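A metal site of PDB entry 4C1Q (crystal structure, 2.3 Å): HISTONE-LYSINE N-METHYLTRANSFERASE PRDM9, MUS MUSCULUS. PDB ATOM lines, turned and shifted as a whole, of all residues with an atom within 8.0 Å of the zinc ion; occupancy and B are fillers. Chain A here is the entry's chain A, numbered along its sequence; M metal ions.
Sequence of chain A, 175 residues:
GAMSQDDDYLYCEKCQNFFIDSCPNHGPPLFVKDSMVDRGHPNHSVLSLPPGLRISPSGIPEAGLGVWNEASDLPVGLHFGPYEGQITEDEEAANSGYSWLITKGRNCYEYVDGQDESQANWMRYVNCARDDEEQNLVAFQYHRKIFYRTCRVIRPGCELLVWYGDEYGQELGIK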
ATOM      1  N   TYR A  11      18.156  -2.428  19.234  1.00  0.00           N
ATOM      2  CA  TYR A  11      16.821  -2.037  18.802  1.00  0.00           C
ATOM      3  C   TYR A  11      16.982  -1.048  17.668  1.00  0.00           C
ATOM      4  O   TYR A  11      17.777  -0.111  17.790  1.00  0.00           O
ATOM      5  CB  TYR A  11      16.070  -1.401  19.972  1.00  0.00           C
ATOM      6  CG  TYR A  11      14.696  -0.887  19.637  1.00  0.00           C
ATOM      7  CD1 TYR A  11      13.624  -1.763  19.427  1.00  0.00           C
ATOM      8  CD2 TYR A  11      14.444   0.482  19.545  1.00  0.00           C
ATOM      9  CE1 TYR A  11      12.352  -1.295  19.140  1.00  0.00           C
ATOM     10  CE2 TYR A  11      13.179   0.958  19.248  1.00  0.00           C
ATOM     11  CZ  TYR A  11      12.142   0.065  19.048  1.00  0.00           C
ATOM     12  OH  TYR A  11      10.900   0.575  18.762  1.00  0.00           O
ATOM     13  N   CYS A  12      16.241  -1.244  16.583  1.00  0.00           N
ATOM     14  CA  CYS A  12      16.206  -0.293  15.476  1.00  0.00           C
ATOM     15  C   CYS A  12      14.997   0.645  15.573  1.00  0.00           C
ATOM     16  O   CYS A  12      13.843   0.190  15.456  1.00  0.00           O
ATOM     17  CB  CYS A  12      16.162  -1.003  14.142  1.00  0.00           C
ATOM     18  SG  CYS A  12      15.901   0.154  12.800  1.00  0.00           S
ATOM     19  N   GLU A  13      15.257   1.941  15.765  1.00  0.00           N
ATOM     20  CA  GLU A  13      14.219   2.977  15.903  1.00  0.00           C
ATOM     21  C   GLU A  13      13.218   2.889  14.748  1.00  0.00           C
ATOM     22  O   GLU A  13      12.016   2.685  14.932  1.00  0.00           O
ATOM     23  CB  GLU A  13      14.848   4.387  15.937  1.00  0.00           C
ATOM     24  CG  GLU A  13      15.804   4.708  17.109  1.00  0.00           C
ATOM     25  CD  GLU A  13      15.092   5.112  18.406  1.00  0.00           C
ATOM     26  OE1 GLU A  13      13.992   5.712  18.373  1.00  0.00           O
ATOM     27  OE2 GLU A  13      15.652   4.851  19.504  1.00  0.00           O
ATOM     28  N   LYS A  14      13.761   2.960  13.537  1.00  0.00           N
ATOM     29  CA  LYS A  14      12.957   3.018  12.327  1.00  0.00           C
ATOM     30  C   LYS A  14      12.059   1.792  12.095  1.00  0.00           C
ATOM     31  O   LYS A  14      10.905   1.943  11.717  1.00  0.00           O
ATOM     32  CB  LYS A  14      13.885   3.239  11.122  1.00  0.00           C
ATOM     33  CG  LYS A  14      14.833   4.426  11.278  1.00  0.00           C
ATOM     34  CD  LYS A  14      15.744   4.588  10.078  1.00  0.00           C
ATOM     35  CE  LYS A  14      16.756   5.704  10.289  1.00  0.00           C
ATOM     36  NZ  LYS A  14      17.912   5.576   9.362  1.00  0.00           N
ATOM     37  N   CYS A  15      12.592   0.596  12.321  1.00  0.00           N
ATOM     38  CA  CYS A  15      11.853  -0.651  12.094  1.00  0.00           C
ATOM     39  C   CYS A  15      11.055  -1.145  13.276  1.00  0.00           C
ATOM     40  O   CYS A  15      10.149  -1.966  13.092  1.00  0.00           O
ATOM     41  CB  CYS A  15      12.817  -1.784  11.780  1.00  0.00           C
ATOM     42  SG  CYS A  15      13.680  -1.529  10.256  1.00  0.00           S
ATOM     43  N   GLN A  16      11.443  -0.729  14.480  1.00  0.00           N
ATOM     44  CA  GLN A  16      10.952  -1.333  15.723  1.00  0.00           C
ATOM     45  C   GLN A  16      11.451  -2.769  15.918  1.00  0.00           C
ATOM     46  O   GLN A  16      10.894  -3.511  16.724  1.00  0.00           O
ATOM     47  CB  GLN A  16       9.417  -1.330  15.775  1.00  0.00           C
ATOM     48  CG  GLN A  16       8.755  -0.069  15.223  1.00  0.00           C
ATOM     49  CD  GLN A  16       8.084   0.778  16.293  1.00  0.00           C
ATOM     50  OE1 GLN A  16       6.965   0.482  16.716  1.00  0.00           O
ATOM     51  NE2 GLN A  16       8.749   1.839  16.720  1.00  0.00           N
ATOM     52  N   ASN A  17      12.496  -3.144  15.182  1.00  0.00           N
ATOM     53  CA  ASN A  17      13.095  -4.491  15.249  1.00  0.00           C
ATOM     54  C   ASN A  17      14.195  -4.601  16.291  1.00  0.00           C
ATOM     55  O   ASN A  17      15.045  -3.736  16.384  1.00  0.00           O
ATOM     56  CB  ASN A  17      13.745  -4.856  13.912  1.00  0.00           C
ATOM     57  CG  ASN A  17      12.746  -5.401  12.932  1.00  0.00           C
ATOM     58  OD1 ASN A  17      11.782  -6.050  13.318  1.00  0.00           O
ATOM     59  ND2 ASN A  17      12.987  -5.146  11.640  1.00  0.00           N
ATOM     60  N   PHE A  18      14.152  -5.679  17.061  1.00  0.00           N
ATOM     61  CA  PHE A  18      15.287  -6.108  17.860  1.00  0.00           C
ATOM     62  C   PHE A  18      16.130  -7.077  17.072  1.00  0.00           C
ATOM     63  O   PHE A  18      15.603  -7.931  16.372  1.00  0.00           O
ATOM     64  CB  PHE A  18      14.819  -6.788  19.141  1.00  0.00           C
ATOM     65  CG  PHE A  18      14.082  -5.884  20.054  1.00  0.00           C
ATOM     66  CD1 PHE A  18      14.770  -5.095  20.963  1.00  0.00           C
ATOM     67  CD2 PHE A  18      12.714  -5.790  19.982  1.00  0.00           C
ATOM     68  CE1 PHE A  18      14.100  -4.227  21.824  1.00  0.00           C
ATOM     69  CE2 PHE A  18      12.025  -4.925  20.819  1.00  0.00           C
ATOM     70  CZ  PHE A  18      12.714  -4.147  21.750  1.00  0.00           C
ATOM     71  N   PHE A  19      17.448  -6.966  17.215  1.00  0.00           N
ATOM     72  CA  PHE A  19      18.379  -7.849  16.535  1.00  0.00           C
ATOM     73  C   PHE A  19      19.669  -7.975  17.319  1.00  0.00           C
ATOM     74  O   PHE A  19      19.962  -7.177  18.195  1.00  0.00           O
ATOM     75  CB  PHE A  19      18.691  -7.278  15.146  1.00  0.00           C
ATOM     76  CG  PHE A  19      19.235  -5.883  15.175  1.00  0.00           C
ATOM     77  CD1 PHE A  19      20.591  -5.653  15.380  1.00  0.00           C
ATOM     78  CD2 PHE A  19      18.407  -4.799  15.008  1.00  0.00           C
ATOM     79  CE1 PHE A  19      21.098  -4.375  15.388  1.00  0.00           C
ATOM     80  CE2 PHE A  19      18.904  -3.515  15.024  1.00  0.00           C
ATOM     81  CZ  PHE A  19      20.261  -3.298  15.200  1.00  0.00           C
ATOM     82  N   SER A  22      22.540  -7.158  13.087  1.00  0.00           N
ATOM     83  CA  SER A  22      22.048  -6.144  12.174  1.00  0.00           C
ATOM     84  C   SER A  22      20.526  -6.117  12.174  1.00  0.00           C
ATOM     85  O   SER A  22      19.888  -7.150  12.265  1.00  0.00           O
ATOM     86  CB  SER A  22      22.502  -6.442  10.755  1.00  0.00           C
ATOM     87  OG  SER A  22      23.909  -6.354  10.662  1.00  0.00           O
ATOM     88  N   CYS A  23      19.945  -4.925  12.072  1.00  0.00           N
ATOM     89  CA  CYS A  23      18.589  -4.816  11.577  1.00  0.00           C
ATOM     90  C   CYS A  23      18.609  -5.427  10.178  1.00  0.00           C
ATOM     91  O   CYS A  23      19.523  -5.142   9.414  1.00  0.00           O
ATOM     92  CB  CYS A  23      18.116  -3.364  11.478  1.00  0.00           C
ATOM     93  SG  CYS A  23      16.409  -3.260  10.889  1.00  0.00           S
ATOM     94  N   PRO A  24      17.632  -6.289   9.852  1.00  0.00           N
ATOM     95  CA  PRO A  24      17.561  -6.855   8.489  1.00  0.00           C
ATOM     96  C   PRO A  24      17.283  -5.809   7.389  1.00  0.00           C
ATOM     97  O   PRO A  24      17.667  -6.004   6.228  1.00  0.00           O
ATOM     98  CB  PRO A  24      16.418  -7.869   8.586  1.00  0.00           C
ATOM     99  CG  PRO A  24      15.666  -7.516   9.820  1.00  0.00           C
ATOM    100  CD  PRO A  24      16.655  -6.913  10.769  1.00  0.00           C
ATOM    101  N   ASN A  25      16.659  -4.691   7.765  1.00  0.00           N
ATOM    102  CA  ASN A  25      16.420  -3.575   6.848  1.00  0.00           C
ATOM    103  C   ASN A  25      17.516  -2.528   6.768  1.00  0.00           C
ATOM    104  O   ASN A  25      17.854  -2.085   5.684  1.00  0.00           O
ATOM    105  CB  ASN A  25      15.129  -2.891   7.268  1.00  0.00           C
ATOM    106  CG  ASN A  25      13.970  -3.856   7.302  1.00  0.00           C
ATOM    107  OD1 ASN A  25      13.765  -4.622   6.367  1.00  0.00           O
ATOM    108  ND2 ASN A  25      13.237  -3.864   8.401  1.00  0.00           N
ATOM    109  N   HIS A  26      18.058  -2.110   7.911  1.00  0.00           N
ATOM    110  CA  HIS A  26      18.980  -0.972   7.955  1.00  0.00           C
ATOM    111  C   HIS A  26      20.443  -1.311   8.220  1.00  0.00           C
ATOM    112  O   HIS A  26      21.278  -0.421   8.244  1.00  0.00           O
ATOM    113  CB  HIS A  26      18.480   0.025   8.986  1.00  0.00           C
ATOM    114  CG  HIS A  26      17.167   0.631   8.628  1.00  0.00           C
ATOM    115  ND1 HIS A  26      15.978  -0.034   8.816  1.00  0.00           N
ATOM    116  CD2 HIS A  26      16.857   1.812   8.068  1.00  0.00           C
ATOM    117  CE1 HIS A  26      14.981   0.728   8.395  1.00  0.00           C
ATOM    118  NE2 HIS A  26      15.483   1.861   7.940  1.00  0.00           N
ATOM    119  N   GLY A  27      20.768  -2.587   8.405  1.00  0.00           N
ATOM    120  CA  GLY A  27      22.154  -2.980   8.652  1.00  0.00           C
ATOM    121  C   GLY A  27      22.564  -2.759  10.108  1.00  0.00           C
ATOM    122  O   GLY A  27      21.735  -2.436  10.959  1.00  0.00           O
HETATM  123 ZN    ZN M   1      15.649  -1.070  11.038  1.00  0.00          ZN
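The side-chain sulfur (SG) of Cys 15 lies close to the side-chain amide nitrogen (ND2) of Asn 25 (3.0 Å).
The backbone NH (N) of Lys 14 sits close to the side-chain sulfur (SG) of Cys 12, at 3.6 Å.
N of Asn 25 lies close to SG of Cys 23 (3.4 Å).
The backbone NH of Cys 12 is in hydrogen-bond range of the backbone carbonyl oxygen of Asn 17.
Along chain A the residues within 4 Å of the zinc ion span positions 12 to 26.
The zinc ion is bound by SG of Cys 12 (2.2 Å), SG of Cys 15 (2.2 Å), SG of Cys 23 (2.3 Å) and ND1 of His 26 (2.5 Å).
The zinc ion has four donor atoms within binding distance.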
